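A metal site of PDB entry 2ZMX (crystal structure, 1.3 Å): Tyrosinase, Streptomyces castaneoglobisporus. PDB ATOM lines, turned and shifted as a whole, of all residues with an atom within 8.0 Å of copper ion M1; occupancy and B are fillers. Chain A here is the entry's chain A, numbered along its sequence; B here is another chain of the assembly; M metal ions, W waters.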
ATOM      1  N   HIS A  38     -11.059   1.599   8.331  1.00  0.00           N
ATOM      2  CA  HIS A  38     -11.151   1.159   9.714  1.00  0.00           C
ATOM      3  C   HIS A  38     -10.412   2.097  10.674  1.00  0.00           C
ATOM      4  O   HIS A  38     -10.906   2.457  11.741  1.00  0.00           O
ATOM      5  CB  HIS A  38     -10.596  -0.273   9.834  1.00  0.00           C
ATOM      6  CG  HIS A  38     -10.849  -0.833  11.216  1.00  0.00           C
ATOM      7  ND1 HIS A  38      -9.908  -0.831  12.207  1.00  0.00           N
ATOM      8  CD2 HIS A  38     -11.964  -1.394  11.769  1.00  0.00           C
ATOM      9  CE1 HIS A  38     -10.389  -1.370  13.304  1.00  0.00           C
ATOM     10  NE2 HIS A  38     -11.631  -1.725  13.061  1.00  0.00           N
ATOM     11  N   ILE A  42     -11.703   4.154  13.944  1.00  0.00           N
ATOM     12  CA  ILE A  42     -11.295   3.880  15.311  1.00  0.00           C
ATOM     13  C   ILE A  42     -10.611   5.080  15.954  1.00  0.00           C
ATOM     14  O   ILE A  42     -10.689   5.296  17.167  1.00  0.00           O
ATOM     15  CB  ILE A  42     -10.421   2.625  15.267  1.00  0.00           C
ATOM     16  CG1 ILE A  42     -10.563   1.824  16.574  1.00  0.00           C
ATOM     17  CG2 ILE A  42      -8.993   2.982  14.915  1.00  0.00           C
ATOM     18  CD1 ILE A  42     -10.145   0.385  16.364  1.00  0.00           C
ATOM     19  N   GLY A  53     -18.263   3.187  14.727  1.00  0.00           N
ATOM     20  CA  GLY A  53     -17.737   1.843  14.426  1.00  0.00           C
ATOM     21  C   GLY A  53     -17.393   1.045  15.654  1.00  0.00           C
ATOM     22  O   GLY A  53     -17.351  -0.194  15.567  1.00  0.00           O
ATOM     23  N   HIS A  54     -17.158   1.685  16.776  1.00  0.00           N
ATOM     24  CA  HIS A  54     -16.628   1.079  17.999  1.00  0.00           C
ATOM     25  C   HIS A  54     -17.219   1.767  19.197  1.00  0.00           C
ATOM     26  O   HIS A  54     -17.769   2.854  19.114  1.00  0.00           O
ATOM     27  CB  HIS A  54     -15.078   1.254  18.107  1.00  0.00           C
ATOM     28  CG  HIS A  54     -14.382   0.716  16.884  1.00  0.00           C
ATOM     29  ND1 HIS A  54     -14.281   1.470  15.715  1.00  0.00           N
ATOM     30  CD2 HIS A  54     -13.845  -0.506  16.669  1.00  0.00           C
ATOM     31  CE1 HIS A  54     -13.653   0.673  14.838  1.00  0.00           C
ATOM     32  NE2 HIS A  54     -13.381  -0.492  15.386  1.00  0.00           N
ATOM     33  N   PHE A  59     -21.248  -0.847  17.054  1.00  0.00           N
ATOM     34  CA  PHE A  59     -20.080  -1.699  16.874  1.00  0.00           C
ATOM     35  C   PHE A  59     -20.402  -2.991  16.136  1.00  0.00           C
ATOM     36  O   PHE A  59     -19.683  -3.342  15.183  1.00  0.00           O
ATOM     37  CB  PHE A  59     -19.487  -2.013  18.252  1.00  0.00           C
ATOM     38  CG  PHE A  59     -18.416  -3.122  18.285  1.00  0.00           C
ATOM     39  CD1 PHE A  59     -17.155  -2.929  17.722  1.00  0.00           C
ATOM     40  CD2 PHE A  59     -18.709  -4.329  18.884  1.00  0.00           C
ATOM     41  CE1 PHE A  59     -16.212  -3.932  17.782  1.00  0.00           C
ATOM     42  CE2 PHE A  59     -17.745  -5.338  18.941  1.00  0.00           C
ATOM     43  CZ  PHE A  59     -16.484  -5.132  18.402  1.00  0.00           C
ATOM     44  N   HIS A  63     -19.526  -3.453  12.036  1.00  0.00           N
ATOM     45  CA  HIS A  63     -18.553  -4.448  11.616  1.00  0.00           C
ATOM     46  C   HIS A  63     -19.208  -5.516  10.738  1.00  0.00           C
ATOM     47  O   HIS A  63     -18.553  -6.087   9.833  1.00  0.00           O
ATOM     48  CB  HIS A  63     -17.820  -5.078  12.816  1.00  0.00           C
ATOM     49  CG  HIS A  63     -16.720  -4.204  13.302  1.00  0.00           C
ATOM     50  ND1 HIS A  63     -16.913  -3.177  14.216  1.00  0.00           N
ATOM     51  CD2 HIS A  63     -15.409  -4.157  12.990  1.00  0.00           C
ATOM     52  CE1 HIS A  63     -15.749  -2.539  14.446  1.00  0.00           C
ATOM     53  NE2 HIS A  63     -14.803  -3.138  13.717  1.00  0.00           N
ATOM     54  N   GLU A 182     -17.570  -6.524  23.115  1.00  0.00           N
ATOM     55  CA  GLU A 182     -16.450  -5.683  22.657  1.00  0.00           C
ATOM     56  C   GLU A 182     -15.252  -5.771  23.567  1.00  0.00           C
ATOM     57  O   GLU A 182     -14.092  -5.901  23.123  1.00  0.00           O
ATOM     58  CB  GLU A 182     -16.983  -4.246  22.470  1.00  0.00           C
ATOM     59  CG  GLU A 182     -16.031  -3.380  21.687  1.00  0.00           C
ATOM     60  CD  GLU A 182     -16.449  -1.976  21.407  1.00  0.00           C
ATOM     61  OE1 GLU A 182     -17.649  -1.668  21.653  1.00  0.00           O
ATOM     62  OE2 GLU A 182     -15.640  -1.160  20.907  1.00  0.00           O
ATOM     63  N   HIS A 190     -13.518  -9.375  22.687  1.00  0.00           N
ATOM     64  CA  HIS A 190     -12.957  -8.917  21.418  1.00  0.00           C
ATOM     65  C   HIS A 190     -11.680  -8.112  21.542  1.00  0.00           C
ATOM     66  O   HIS A 190     -10.726  -8.300  20.763  1.00  0.00           O
ATOM     67  CB  HIS A 190     -14.042  -8.110  20.654  1.00  0.00           C
ATOM     68  CG  HIS A 190     -13.495  -7.043  19.742  1.00  0.00           C
ATOM     69  ND1 HIS A 190     -13.213  -5.781  20.172  1.00  0.00           N
ATOM     70  CD2 HIS A 190     -13.230  -7.055  18.428  1.00  0.00           C
ATOM     71  CE1 HIS A 190     -12.749  -5.040  19.156  1.00  0.00           C
ATOM     72  NE2 HIS A 190     -12.747  -5.830  18.074  1.00  0.00           N
ATOM     73  N   ASN A 191     -11.615  -7.159  22.511  1.00  0.00           N
ATOM     74  CA  ASN A 191     -10.390  -6.375  22.621  1.00  0.00           C
ATOM     75  C   ASN A 191      -9.206  -7.265  22.989  1.00  0.00           C
ATOM     76  O   ASN A 191      -8.099  -7.077  22.473  1.00  0.00           O
ATOM     77  CB  ASN A 191     -10.500  -5.276  23.683  1.00  0.00           C
ATOM     78  CG  ASN A 191     -11.418  -4.137  23.256  1.00  0.00           C
ATOM     79  OD1 ASN A 191     -11.850  -4.060  22.111  1.00  0.00           O
ATOM     80  ND2 ASN A 191     -11.693  -3.237  24.198  1.00  0.00           N
ATOM     81  N   VAL A 193      -8.643 -10.337  22.241  1.00  0.00           N
ATOM     82  CA  VAL A 193      -8.037 -11.069  21.116  1.00  0.00           C
ATOM     83  C   VAL A 193      -7.122 -10.177  20.302  1.00  0.00           C
ATOM     84  O   VAL A 193      -6.048 -10.642  19.872  1.00  0.00           O
ATOM     85  CB  VAL A 193      -9.150 -11.636  20.240  1.00  0.00           C
ATOM     86  CG1 VAL A 193      -8.551 -12.327  19.012  1.00  0.00           C
ATOM     87  CG2 VAL A 193      -9.988 -12.610  21.046  1.00  0.00           C
ATOM     88  N   HIS A 194      -7.513  -8.916  20.045  1.00  0.00           N
ATOM     89  CA  HIS A 194      -6.593  -8.030  19.364  1.00  0.00           C
ATOM     90  C   HIS A 194      -5.249  -7.911  20.080  1.00  0.00           C
ATOM     91  O   HIS A 194      -4.151  -7.905  19.488  1.00  0.00           O
ATOM     92  CB  HIS A 194      -7.172  -6.615  19.220  1.00  0.00           C
ATOM     93  CG  HIS A 194      -8.173  -6.399  18.130  1.00  0.00           C
ATOM     94  ND1 HIS A 194      -7.793  -6.074  16.826  1.00  0.00           N
ATOM     95  CD2 HIS A 194      -9.528  -6.379  18.153  1.00  0.00           C
ATOM     96  CE1 HIS A 194      -8.907  -5.918  16.140  1.00  0.00           C
ATOM     97  NE2 HIS A 194     -10.024  -6.069  16.869  1.00  0.00           N
ATOM     98  N   MET A 201      -2.355  -6.068  14.463  1.00  0.00           N
ATOM     99  CA  MET A 201      -3.677  -6.386  15.030  1.00  0.00           C
ATOM    100  C   MET A 201      -3.947  -5.680  16.339  1.00  0.00           C
ATOM    101  O   MET A 201      -5.135  -5.541  16.696  1.00  0.00           O
ATOM    102  CB  MET A 201      -3.716  -7.909  15.179  1.00  0.00           C
ATOM    103  CG  MET A 201      -5.046  -8.517  15.406  1.00  0.00           C
ATOM    104  SD  MET A 201      -6.345  -8.179  14.202  1.00  0.00           S
ATOM    105  CE  MET A 201      -7.616  -9.164  15.051  1.00  0.00           C
ATOM    106  N   THR A 203      -3.240  -2.549  16.938  1.00  0.00           N
ATOM    107  CA  THR A 203      -3.243  -1.125  16.608  1.00  0.00           C
ATOM    108  C   THR A 203      -4.479  -0.664  15.862  1.00  0.00           C
ATOM    109  O   THR A 203      -5.349  -1.459  15.507  1.00  0.00           O
ATOM    110  CB  THR A 203      -2.009  -0.737  15.757  1.00  0.00           C
ATOM    111  OG1 THR A 203      -2.259  -1.210  14.412  1.00  0.00           O
ATOM    112  CG2 THR A 203      -0.762  -1.375  16.326  1.00  0.00           C
ATOM    113  N   SER A 206      -5.455  -2.406  12.415  1.00  0.00           N
ATOM    114  CA  SER A 206      -5.500  -3.855  12.588  1.00  0.00           C
ATOM    115  C   SER A 206      -5.983  -4.637  11.369  1.00  0.00           C
ATOM    116  O   SER A 206      -5.534  -5.795  11.286  1.00  0.00           O
ATOM    117  CB  SER A 206      -6.394  -4.202  13.803  1.00  0.00           C
ATOM    118  OG  SER A 206      -7.666  -3.584  13.714  1.00  0.00           O
ATOM    119  N   PRO A 207      -6.793  -4.145  10.438  1.00  0.00           N
ATOM    120  CA  PRO A 207      -7.041  -4.977   9.235  1.00  0.00           C
ATOM    121  C   PRO A 207      -5.784  -5.214   8.401  1.00  0.00           C
ATOM    122  O   PRO A 207      -5.882  -6.029   7.460  1.00  0.00           O
ATOM    123  CB  PRO A 207      -8.072  -4.146   8.443  1.00  0.00           C
ATOM    124  CG  PRO A 207      -8.769  -3.374   9.552  1.00  0.00           C
ATOM    125  CD  PRO A 207      -7.609  -2.916  10.400  1.00  0.00           C
ATOM    126  N   PHE A 212      -7.711 -10.289  11.078  1.00  0.00           N
ATOM    127  CA  PHE A 212      -8.767  -9.380  11.480  1.00  0.00           C
ATOM    128  C   PHE A 212     -10.156  -9.864  11.094  1.00  0.00           C
ATOM    129  O   PHE A 212     -11.121  -9.747  11.833  1.00  0.00           O
ATOM    130  CB  PHE A 212      -8.508  -8.014  10.792  1.00  0.00           C
ATOM    131  CG  PHE A 212      -9.550  -6.960  11.033  1.00  0.00           C
ATOM    132  CD1 PHE A 212     -10.669  -6.806  10.201  1.00  0.00           C
ATOM    133  CD2 PHE A 212      -9.427  -6.098  12.126  1.00  0.00           C
ATOM    134  CE1 PHE A 212     -11.635  -5.885  10.477  1.00  0.00           C
ATOM    135  CE2 PHE A 212     -10.417  -5.153  12.363  1.00  0.00           C
ATOM    136  CZ  PHE A 212     -11.530  -5.051  11.545  1.00  0.00           C
ATOM    137  N   HIS A 215     -11.313 -13.004  13.071  1.00  0.00           N
ATOM    138  CA  HIS A 215     -11.712 -12.566  14.413  1.00  0.00           C
ATOM    139  C   HIS A 215     -13.100 -11.936  14.346  1.00  0.00           C
ATOM    140  O   HIS A 215     -14.035 -12.363  15.056  1.00  0.00           O
ATOM    141  CB  HIS A 215     -10.662 -11.585  14.935  1.00  0.00           C
ATOM    142  CG  HIS A 215     -11.010 -10.957  16.261  1.00  0.00           C
ATOM    143  ND1 HIS A 215     -11.693 -11.669  17.207  1.00  0.00           N
ATOM    144  CD2 HIS A 215     -10.757  -9.718  16.752  1.00  0.00           C
ATOM    145  CE1 HIS A 215     -11.851 -10.881  18.271  1.00  0.00           C
ATOM    146  NE2 HIS A 215     -11.310  -9.707  18.027  1.00  0.00           N
ATOM    147  N   HIS A 216     -13.278 -10.900  13.500  1.00  0.00           N
ATOM    148  CA  HIS A 216     -14.573 -10.242  13.477  1.00  0.00           C
ATOM    149  C   HIS A 216     -15.660 -11.145  12.935  1.00  0.00           C
ATOM    150  O   HIS A 216     -16.829 -10.927  13.361  1.00  0.00           O
ATOM    151  CB  HIS A 216     -14.474  -8.906  12.697  1.00  0.00           C
ATOM    152  CG  HIS A 216     -14.084  -7.828  13.668  1.00  0.00           C
ATOM    153  ND1 HIS A 216     -15.023  -7.192  14.474  1.00  0.00           N
ATOM    154  CD2 HIS A 216     -12.900  -7.272  14.009  1.00  0.00           C
ATOM    155  CE1 HIS A 216     -14.399  -6.314  15.255  1.00  0.00           C
ATOM    156  NE2 HIS A 216     -13.097  -6.326  14.993  1.00  0.00           N
ATOM    157  N   VAL A 219     -16.747 -12.779  16.155  1.00  0.00           N
ATOM    158  CA  VAL A 219     -17.516 -11.821  16.957  1.00  0.00           C
ATOM    159  C   VAL A 219     -18.900 -11.690  16.399  1.00  0.00           C
ATOM    160  O   VAL A 219     -19.898 -11.610  17.149  1.00  0.00           O
ATOM    161  CB  VAL A 219     -16.783 -10.468  16.982  1.00  0.00           C
ATOM    162  CG1 VAL A 219     -17.616  -9.334  17.588  1.00  0.00           C
ATOM    163  CG2 VAL A 219     -15.465 -10.590  17.736  1.00  0.00           C
ATOM    164  N   HIS B  97      -4.438   0.140  20.700  1.00  0.00           N
ATOM    165  CA  HIS B  97      -5.761   0.762  20.713  1.00  0.00           C
ATOM    166  C   HIS B  97      -6.704  -0.037  21.579  1.00  0.00           C
ATOM    167  O   HIS B  97      -7.747   0.454  22.027  1.00  0.00           O
ATOM    168  CB  HIS B  97      -6.297   0.850  19.276  1.00  0.00           C
ATOM    169  CG  HIS B  97      -7.669   1.449  19.341  1.00  0.00           C
ATOM    170  ND1 HIS B  97      -7.795   2.818  19.379  1.00  0.00           N
ATOM    171  CD2 HIS B  97      -8.931   0.963  19.380  1.00  0.00           C
ATOM    172  CE1 HIS B  97      -9.056   3.149  19.441  1.00  0.00           C
ATOM    173  NE2 HIS B  97      -9.767   2.048  19.446  1.00  0.00           N
ATOM    174  N   TYR B  98      -6.400  -1.301  21.812  1.00  0.00           N
ATOM    175  CA  TYR B  98      -7.419  -2.149  22.462  1.00  0.00           C
ATOM    176  C   TYR B  98      -7.011  -2.488  23.880  1.00  0.00           C
ATOM    177  O   TYR B  98      -7.487  -3.456  24.480  1.00  0.00           O
ATOM    178  CB  TYR B  98      -7.636  -3.408  21.619  1.00  0.00           C
ATOM    179  CG  TYR B  98      -7.984  -3.182  20.166  1.00  0.00           C
ATOM    180  CD1 TYR B  98      -7.033  -3.114  19.155  1.00  0.00           C
ATOM    181  CD2 TYR B  98      -9.324  -3.027  19.775  1.00  0.00           C
ATOM    182  CE1 TYR B  98      -7.360  -2.908  17.828  1.00  0.00           C
ATOM    183  CE2 TYR B  98      -9.630  -2.821  18.456  1.00  0.00           C
ATOM    184  CZ  TYR B  98      -8.678  -2.754  17.478  1.00  0.00           C
ATOM    185  OH  TYR B  98      -9.035  -2.568  16.145  1.00  0.00           O
HETATM  186 CU    CU M   1     -11.836  -5.350  16.356  1.00  0.00          CU
HETATM  187 CU    CU M   2     -12.780  -2.215  14.593  1.00  0.00          CU
HETATM  188  O   HOH W   1     -11.405  -3.808  15.259  1.00  0.00           O
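O of His 190 lies within hydrogen-bond range of NE2 of His 215, at 3.1 Å. A ring nitrogen (ND1) of His 190 is in hydrogen-bond range of the side-chain amide oxygen (OD1) of Asn 191, at 2.9 Å. The backbone carbonyl oxygen (O) of Glu 182 is in hydrogen-bond range of a ring nitrogen (ND1) of His 190 (3.1 Å). A ring nitrogen (ND1) of His 194 is in hydrogen-bond range of the backbone carbonyl oxygen (O) of Met 201 (2.7 Å). The side-chain hydroxyl of Ser 206 lies within hydrogen-bond range of the side-chain hydroxyl of Tyr 98 of chain B (3.0 Å).
Copper ion M1 is bound by water W1 (1.9 Å), NE2 of His 190 (2.0 Å), NE2 of His 194 (2.0 Å) and NE2 of His 216 (2.1 Å). Copper ion M1 has four donor atoms within binding distance.
Tyr 98 of chain B touches copper ion M1. Within 4 Å of copper ion M1: His 190, His 194, His 216 and Tyr 98 of chain B. The nearest printed residue that does not touch copper ion M1 is Phe 212 (4.2 Å).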
